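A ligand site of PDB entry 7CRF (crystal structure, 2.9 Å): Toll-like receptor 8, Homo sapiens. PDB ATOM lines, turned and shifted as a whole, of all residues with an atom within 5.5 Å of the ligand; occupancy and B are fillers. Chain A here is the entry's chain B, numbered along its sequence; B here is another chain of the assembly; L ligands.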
ATOM      1  N   PHE A 472      12.889  24.528  -7.338  1.00  0.00           N
ATOM      2  CA  PHE A 472      12.307  23.819  -6.169  1.00  0.00           C
ATOM      3  C   PHE A 472      11.744  24.844  -5.174  1.00  0.00           C
ATOM      4  O   PHE A 472      10.785  24.538  -4.464  1.00  0.00           O
ATOM      5  CB  PHE A 472      13.302  22.816  -5.574  1.00  0.00           C
ATOM      6  CG  PHE A 472      14.311  23.355  -4.583  1.00  0.00           C
ATOM      7  CD1 PHE A 472      15.620  23.583  -4.964  1.00  0.00           C
ATOM      8  CD2 PHE A 472      13.953  23.582  -3.260  1.00  0.00           C
ATOM      9  CE1 PHE A 472      16.554  24.043  -4.052  1.00  0.00           C
ATOM     10  CE2 PHE A 472      14.887  24.042  -2.348  1.00  0.00           C
ATOM     11  CZ  PHE A 472      16.183  24.280  -2.747  1.00  0.00           C
ATOM     12  N   PHE A 473      12.327  26.039  -5.139  1.00  0.00           N
ATOM     13  CA  PHE A 473      11.664  27.255  -4.584  1.00  0.00           C
ATOM     14  C   PHE A 473      11.978  28.423  -5.514  1.00  0.00           C
ATOM     15  O   PHE A 473      13.045  28.409  -6.183  1.00  0.00           O
ATOM     16  CB  PHE A 473      12.074  27.519  -3.130  1.00  0.00           C
ATOM     17  CG  PHE A 473      13.413  28.191  -2.931  1.00  0.00           C
ATOM     18  CD1 PHE A 473      13.492  29.475  -2.435  1.00  0.00           C
ATOM     19  CD2 PHE A 473      14.591  27.516  -3.227  1.00  0.00           C
ATOM     20  CE1 PHE A 473      14.724  30.097  -2.258  1.00  0.00           C
ATOM     21  CE2 PHE A 473      15.822  28.138  -3.050  1.00  0.00           C
ATOM     22  CZ  PHE A 473      15.884  29.419  -2.571  1.00  0.00           C
ATOM     23  N   ALA A 496       7.913  22.781  -3.662  1.00  0.00           N
ATOM     24  CA  ALA A 496       7.165  22.372  -2.454  1.00  0.00           C
ATOM     25  C   ALA A 496       7.245  23.476  -1.397  1.00  0.00           C
ATOM     26  O   ALA A 496       7.457  23.157  -0.221  1.00  0.00           O
ATOM     27  CB  ALA A 496       7.719  21.055  -1.961  1.00  0.00           C
ATOM     28  N   GLN A 497       7.033  24.729  -1.819  1.00  0.00           N
ATOM     29  CA  GLN A 497       7.391  25.932  -1.032  1.00  0.00           C
ATOM     30  C   GLN A 497       6.137  26.607  -0.460  1.00  0.00           C
ATOM     31  O   GLN A 497       5.029  26.402  -0.989  1.00  0.00           O
ATOM     32  CB  GLN A 497       8.172  26.929  -1.896  1.00  0.00           C
ATOM     33  CG  GLN A 497       7.312  27.922  -2.655  1.00  0.00           C
ATOM     34  CD  GLN A 497       8.116  29.086  -3.182  1.00  0.00           C
ATOM     35  OE1 GLN A 497       8.818  28.997  -4.188  1.00  0.00           O
ATOM     36  NE2 GLN A 497       7.998  30.208  -2.491  1.00  0.00           N
ATOM     37  N   VAL A 498       6.347  27.388   0.604  1.00  0.00           N
ATOM     38  CA  VAL A 498       5.398  28.388   1.144  1.00  0.00           C
ATOM     39  C   VAL A 498       5.494  29.627   0.245  1.00  0.00           C
ATOM     40  O   VAL A 498       6.592  29.896  -0.282  1.00  0.00           O
ATOM     41  CB  VAL A 498       5.703  28.723   2.609  1.00  0.00           C
ATOM     42  CG1 VAL A 498       5.061  30.036   3.054  1.00  0.00           C
ATOM     43  CG2 VAL A 498       5.286  27.593   3.523  1.00  0.00           C
ATOM     44  N   ASP A 521       2.737  24.682  -0.545  1.00  0.00           N
ATOM     45  CA  ASP A 521       2.101  24.812   0.786  1.00  0.00           C
ATOM     46  C   ASP A 521       1.325  26.130   0.838  1.00  0.00           C
ATOM     47  O   ASP A 521       1.968  27.178   1.058  1.00  0.00           O
ATOM     48  CB  ASP A 521       3.131  24.714   1.902  1.00  0.00           C
ATOM     49  CG  ASP A 521       2.513  24.567   3.284  1.00  0.00           C
ATOM     50  OD1 ASP A 521       3.283  24.467   4.265  1.00  0.00           O
ATOM     51  OD2 ASP A 521       1.262  24.543   3.363  1.00  0.00           O
ATOM     52  N   TYR A 545       0.202  19.039   0.490  1.00  0.00           N
ATOM     53  CA  TYR A 545       0.071  19.816   1.759  1.00  0.00           C
ATOM     54  C   TYR A 545      -1.406  20.002   2.112  1.00  0.00           C
ATOM     55  O   TYR A 545      -1.704  20.253   3.300  1.00  0.00           O
ATOM     56  CB  TYR A 545       0.834  21.139   1.687  1.00  0.00           C
ATOM     57  CG  TYR A 545       2.307  21.027   2.008  1.00  0.00           C
ATOM     58  CD1 TYR A 545       3.266  21.104   1.015  1.00  0.00           C
ATOM     59  CD2 TYR A 545       2.743  20.796   3.310  1.00  0.00           C
ATOM     60  CE1 TYR A 545       4.618  20.975   1.292  1.00  0.00           C
ATOM     61  CE2 TYR A 545       4.092  20.669   3.595  1.00  0.00           C
ATOM     62  CZ  TYR A 545       5.034  20.758   2.594  1.00  0.00           C
ATOM     63  OH  TYR A 545       6.359  20.646   2.889  1.00  0.00           O
ATOM     64  N   VAL A 551      -0.480  21.470   9.021  1.00  0.00           N
ATOM     65  CA  VAL A 551      -0.227  22.648   8.163  1.00  0.00           C
ATOM     66  C   VAL A 551      -1.582  23.339   7.937  1.00  0.00           C
ATOM     67  O   VAL A 551      -2.580  22.616   7.786  1.00  0.00           O
ATOM     68  CB  VAL A 551       0.451  22.195   6.859  1.00  0.00           C
ATOM     69  CG1 VAL A 551      -0.086  22.902   5.630  1.00  0.00           C
ATOM     70  CG2 VAL A 551       1.969  22.325   6.930  1.00  0.00           C
ATOM     71  N   CYS B 238       5.885  23.623  12.431  1.00  0.00           N
ATOM     72  CA  CYS B 238       5.021  22.920  11.443  1.00  0.00           C
ATOM     73  C   CYS B 238       5.851  22.493  10.227  1.00  0.00           C
ATOM     74  O   CYS B 238       6.737  23.268   9.810  1.00  0.00           O
ATOM     75  CB  CYS B 238       3.872  23.812  10.995  1.00  0.00           C
ATOM     76  SG  CYS B 238       2.669  24.178  12.306  1.00  0.00           S
ATOM     77  N   PHE B 239       5.566  21.299   9.675  1.00  0.00           N
ATOM     78  CA  PHE B 239       6.110  20.807   8.380  1.00  0.00           C
ATOM     79  C   PHE B 239       5.172  19.767   7.737  1.00  0.00           C
ATOM     80  O   PHE B 239       4.407  20.163   6.840  1.00  0.00           O
ATOM     81  CB  PHE B 239       7.545  20.287   8.549  1.00  0.00           C
ATOM     82  CG  PHE B 239       8.268  20.102   7.242  1.00  0.00           C
ATOM     83  CD1 PHE B 239       8.390  18.839   6.668  1.00  0.00           C
ATOM     84  CD2 PHE B 239       8.827  21.183   6.569  1.00  0.00           C
ATOM     85  CE1 PHE B 239       9.040  18.669   5.461  1.00  0.00           C
ATOM     86  CE2 PHE B 239       9.489  20.995   5.359  1.00  0.00           C
ATOM     87  CZ  PHE B 239       9.595  19.746   4.809  1.00  0.00           C
ATOM     88  N   PHE B 324      15.417  18.894   9.262  1.00  0.00           N
ATOM     89  CA  PHE B 324      14.409  19.969   9.075  1.00  0.00           C
ATOM     90  C   PHE B 324      14.615  21.069  10.117  1.00  0.00           C
ATOM     91  O   PHE B 324      13.652  21.467  10.794  1.00  0.00           O
ATOM     92  CB  PHE B 324      13.002  19.363   9.066  1.00  0.00           C
ATOM     93  CG  PHE B 324      12.780  18.487   7.863  1.00  0.00           C
ATOM     94  CD1 PHE B 324      12.685  19.052   6.597  1.00  0.00           C
ATOM     95  CD2 PHE B 324      12.709  17.106   7.980  1.00  0.00           C
ATOM     96  CE1 PHE B 324      12.505  18.244   5.484  1.00  0.00           C
ATOM     97  CE2 PHE B 324      12.517  16.316   6.870  1.00  0.00           C
ATOM     98  CZ  PHE B 324      12.423  16.875   5.616  1.00  0.00           C
ATOM     99  N   TYR B 326      16.334  23.774   8.714  1.00  0.00           N
ATOM    100  CA  TYR B 326      16.518  24.811   7.671  1.00  0.00           C
ATOM    101  C   TYR B 326      15.947  26.155   8.138  1.00  0.00           C
ATOM    102  O   TYR B 326      14.937  26.164   8.874  1.00  0.00           O
ATOM    103  CB  TYR B 326      15.828  24.408   6.363  1.00  0.00           C
ATOM    104  CG  TYR B 326      14.318  24.404   6.423  1.00  0.00           C
ATOM    105  CD1 TYR B 326      13.619  23.280   6.831  1.00  0.00           C
ATOM    106  CD2 TYR B 326      13.586  25.530   6.082  1.00  0.00           C
ATOM    107  CE1 TYR B 326      12.237  23.274   6.908  1.00  0.00           C
ATOM    108  CE2 TYR B 326      12.199  25.539   6.144  1.00  0.00           C
ATOM    109  CZ  TYR B 326      11.521  24.416   6.560  1.00  0.00           C
ATOM    110  OH  TYR B 326      10.154  24.412   6.622  1.00  0.00           O
ATOM    111  N   ILE B 327      16.601  27.256   7.728  1.00  0.00           N
ATOM    112  CA  ILE B 327      16.050  28.637   7.781  1.00  0.00           C
ATOM    113  C   ILE B 327      15.238  28.853   6.486  1.00  0.00           C
ATOM    114  O   ILE B 327      15.846  28.743   5.392  1.00  0.00           O
ATOM    115  CB  ILE B 327      17.169  29.688   7.958  1.00  0.00           C
ATOM    116  CG1 ILE B 327      17.840  29.575   9.329  1.00  0.00           C
ATOM    117  CG2 ILE B 327      16.650  31.096   7.711  1.00  0.00           C
ATOM    118  CD1 ILE B 327      19.259  30.112   9.356  1.00  0.00           C
ATOM    119  N   LYS B 328      13.941  29.138   6.627  1.00  0.00           N
ATOM    120  CA  LYS B 328      13.011  29.396   5.496  1.00  0.00           C
ATOM    121  C   LYS B 328      13.612  30.420   4.534  1.00  0.00           C
ATOM    122  O   LYS B 328      13.821  31.569   4.977  1.00  0.00           O
ATOM    123  CB  LYS B 328      11.662  29.905   6.031  1.00  0.00           C
ATOM    124  CG  LYS B 328      10.579  30.046   4.973  1.00  0.00           C
ATOM    125  CD  LYS B 328       9.461  30.990   5.337  1.00  0.00           C
ATOM    126  CE  LYS B 328       9.010  30.861   6.770  1.00  0.00           C
ATOM    127  NZ  LYS B 328       7.840  31.752   7.005  1.00  0.00           N
ATOM    128  N   GLY B 329      13.885  30.017   3.289  1.00  0.00           N
ATOM    129  CA  GLY B 329      14.323  30.926   2.209  1.00  0.00           C
ATOM    130  C   GLY B 329      15.829  30.984   2.049  1.00  0.00           C
ATOM    131  O   GLY B 329      16.297  31.494   1.027  1.00  0.00           O
ATOM    132  N   SER B 330      16.569  30.485   3.043  1.00  0.00           N
ATOM    133  CA  SER B 330      18.057  30.456   3.047  1.00  0.00           C
ATOM    134  C   SER B 330      18.553  29.184   2.349  1.00  0.00           C
ATOM    135  O   SER B 330      18.377  28.109   2.922  1.00  0.00           O
ATOM    136  CB  SER B 330      18.597  30.564   4.453  1.00  0.00           C
ATOM    137  OG  SER B 330      19.997  30.268   4.486  1.00  0.00           O
ATOM    138  N   TYR B 331      19.181  29.337   1.178  1.00  0.00           N
ATOM    139  CA  TYR B 331      19.835  28.233   0.411  1.00  0.00           C
ATOM    140  C   TYR B 331      21.350  28.425   0.490  1.00  0.00           C
ATOM    141  O   TYR B 331      22.010  28.630  -0.526  1.00  0.00           O
ATOM    142  CB  TYR B 331      19.278  28.225  -1.022  1.00  0.00           C
ATOM    143  CG  TYR B 331      19.608  27.023  -1.876  1.00  0.00           C
ATOM    144  CD1 TYR B 331      19.948  25.799  -1.332  1.00  0.00           C
ATOM    145  CD2 TYR B 331      19.518  27.111  -3.253  1.00  0.00           C
ATOM    146  CE1 TYR B 331      20.216  24.701  -2.144  1.00  0.00           C
ATOM    147  CE2 TYR B 331      19.786  26.036  -4.069  1.00  0.00           C
ATOM    148  CZ  TYR B 331      20.131  24.817  -3.514  1.00  0.00           C
ATOM    149  OH  TYR B 331      20.391  23.759  -4.337  1.00  0.00           O
ATOM    150  N   TYR B 355      18.301  20.540   5.884  1.00  0.00           N
ATOM    151  CA  TYR B 355      19.114  21.713   6.299  1.00  0.00           C
ATOM    152  C   TYR B 355      19.072  22.717   5.152  1.00  0.00           C
ATOM    153  O   TYR B 355      18.905  23.925   5.401  1.00  0.00           O
ATOM    154  CB  TYR B 355      20.547  21.303   6.631  1.00  0.00           C
ATOM    155  CG  TYR B 355      21.436  22.427   7.096  1.00  0.00           C
ATOM    156  CD1 TYR B 355      22.022  23.304   6.201  1.00  0.00           C
ATOM    157  CD2 TYR B 355      21.724  22.587   8.436  1.00  0.00           C
ATOM    158  CE1 TYR B 355      22.862  24.328   6.624  1.00  0.00           C
ATOM    159  CE2 TYR B 355      22.549  23.603   8.888  1.00  0.00           C
ATOM    160  CZ  TYR B 355      23.126  24.482   7.977  1.00  0.00           C
ATOM    161  OH  TYR B 355      23.940  25.473   8.440  1.00  0.00           O
ATOM    162  N   VAL B 356      19.234  22.187   3.933  1.00  0.00           N
ATOM    163  CA  VAL B 356      19.062  22.885   2.620  1.00  0.00           C
ATOM    164  C   VAL B 356      20.307  23.729   2.353  1.00  0.00           C
ATOM    165  O   VAL B 356      20.395  24.851   2.907  1.00  0.00           O
ATOM    166  CB  VAL B 356      17.792  23.770   2.575  1.00  0.00           C
ATOM    167  CG1 VAL B 356      17.645  24.411   1.207  1.00  0.00           C
ATOM    168  CG2 VAL B 356      16.533  22.998   2.953  1.00  0.00           C
ATOM    169  N   ILE B 381      17.082  15.239   1.202  1.00  0.00           N
ATOM    170  CA  ILE B 381      16.245  16.456   1.043  1.00  0.00           C
ATOM    171  C   ILE B 381      17.068  17.687   1.472  1.00  0.00           C
ATOM    172  O   ILE B 381      16.594  18.422   2.340  1.00  0.00           O
ATOM    173  CB  ILE B 381      14.947  16.325   1.868  1.00  0.00           C
ATOM    174  CG1 ILE B 381      14.387  14.896   1.779  1.00  0.00           C
ATOM    175  CG2 ILE B 381      13.911  17.354   1.449  1.00  0.00           C
ATOM    176  CD1 ILE B 381      13.243  14.614   2.718  1.00  0.00           C
ATOM    177  N   PHE B 383      18.866  19.305  -1.292  1.00  0.00           N
ATOM    178  CA  PHE B 383      18.933  19.964  -2.611  1.00  0.00           C
ATOM    179  C   PHE B 383      20.386  20.345  -2.933  1.00  0.00           C
ATOM    180  O   PHE B 383      20.633  21.368  -3.609  1.00  0.00           O
ATOM    181  CB  PHE B 383      17.984  21.173  -2.649  1.00  0.00           C
ATOM    182  CG  PHE B 383      16.567  20.838  -2.256  1.00  0.00           C
ATOM    183  CD1 PHE B 383      15.657  20.392  -3.194  1.00  0.00           C
ATOM    184  CD2 PHE B 383      16.147  20.974  -0.940  1.00  0.00           C
ATOM    185  CE1 PHE B 383      14.350  20.087  -2.830  1.00  0.00           C
ATOM    186  CE2 PHE B 383      14.853  20.665  -0.570  1.00  0.00           C
ATOM    187  CZ  PHE B 383      13.954  20.222  -1.515  1.00  0.00           C
HETATM  188  C1  LIG L   1      12.803  27.022   1.755  1.00  0.00           C
HETATM  189  N1  LIG L   1       9.129  27.529   1.447  1.00  0.00           N
HETATM  190  O1  LIG L   1       8.265  24.760   3.486  1.00  0.00           O
HETATM  191  C2  LIG L   1      14.927  27.360   0.701  1.00  0.00           C
HETATM  192  C3  LIG L   1      13.414  26.584   2.915  1.00  0.00           C
HETATM  193  C4  LIG L   1      15.542  26.950   1.868  1.00  0.00           C
HETATM  194  C5  LIG L   1      14.798  26.562   2.975  1.00  0.00           C
HETATM  195  C6  LIG L   1      11.346  27.016   1.715  1.00  0.00           C
HETATM  196  C7  LIG L   1      10.352  28.064   1.320  1.00  0.00           C
HETATM  197  C8  LIG L   1       9.336  26.240   1.874  1.00  0.00           C
HETATM  198  C9  LIG L   1      11.085  24.617   2.508  1.00  0.00           C
HETATM  199  C10 LIG L   1      11.525  23.528   1.533  1.00  0.00           C
HETATM  200  C11 LIG L   1      12.590  24.065   0.589  1.00  0.00           C
HETATM  201  C12 LIG L   1      12.077  22.349   2.294  1.00  0.00           C
HETATM  202  C13 LIG L   1       8.252  25.242   2.148  1.00  0.00           C
HETATM  203  C14 LIG L   1       6.904  24.649   3.932  1.00  0.00           C
HETATM  204  I1  LIG L   1      10.623  30.121   0.665  1.00  0.00           I
HETATM  205  C15 LIG L   1       6.785  23.664   5.056  1.00  0.00           C
HETATM  206  N2  LIG L   1      10.629  25.918   2.002  1.00  0.00           N
HETATM  207  O2  LIG L   1      10.427  23.006   0.787  1.00  0.00           O
HETATM  208  C16 LIG L   1      13.539  27.390   0.637  1.00  0.00           C
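The backbone NH of Val 498 sits at hydrogen-bond distance from a nitrogen (N1) of the ligand (2.9 Å). An oxygen (O2) of the ligand is in hydrogen-bond range of the backbone carbonyl oxygen (O) of Ala 496, 3.1 Å away.
The backbone carbonyl oxygen (O) of Phe 472 lies within hydrogen-bond range of the backbone NH (N) of Ala 496 (3.5 Å). The backbone carbonyl oxygen (O) of Gln 497 is in hydrogen-bond range of the backbone NH (N) of Asp 521, 2.9 Å away.
Phe 472 touches the ligand. CG of Phe 473 touches C16 of the ligand, at 3.7 Å. Gln 497 touches the ligand. OD1 of Asp 521 touches C14 of the ligand, at 3.6 Å. OH of Tyr 545 touches C15 of the ligand, at 3.7 Å. Phe 239 of chain B touches the ligand (CD2 to C15, 3.6 Å). Tyr 326 of chain B touches the ligand. Ile 327 of chain B touches the ligand (O to C5, 3.4 Å). Lys 328 of chain B touches the ligand (CA to C3, 3.8 Å). N of Gly 329 of chain B touches C3 of the ligand, 3.5 Å away. O of Ser 330 of chain B touches C4 of the ligand, at 3.2 Å. CG1 of Val 356 of chain B touches C4 of the ligand, 3.4 Å away. Of the 21 residues printed, 14 come within 4 Å of the ligand.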
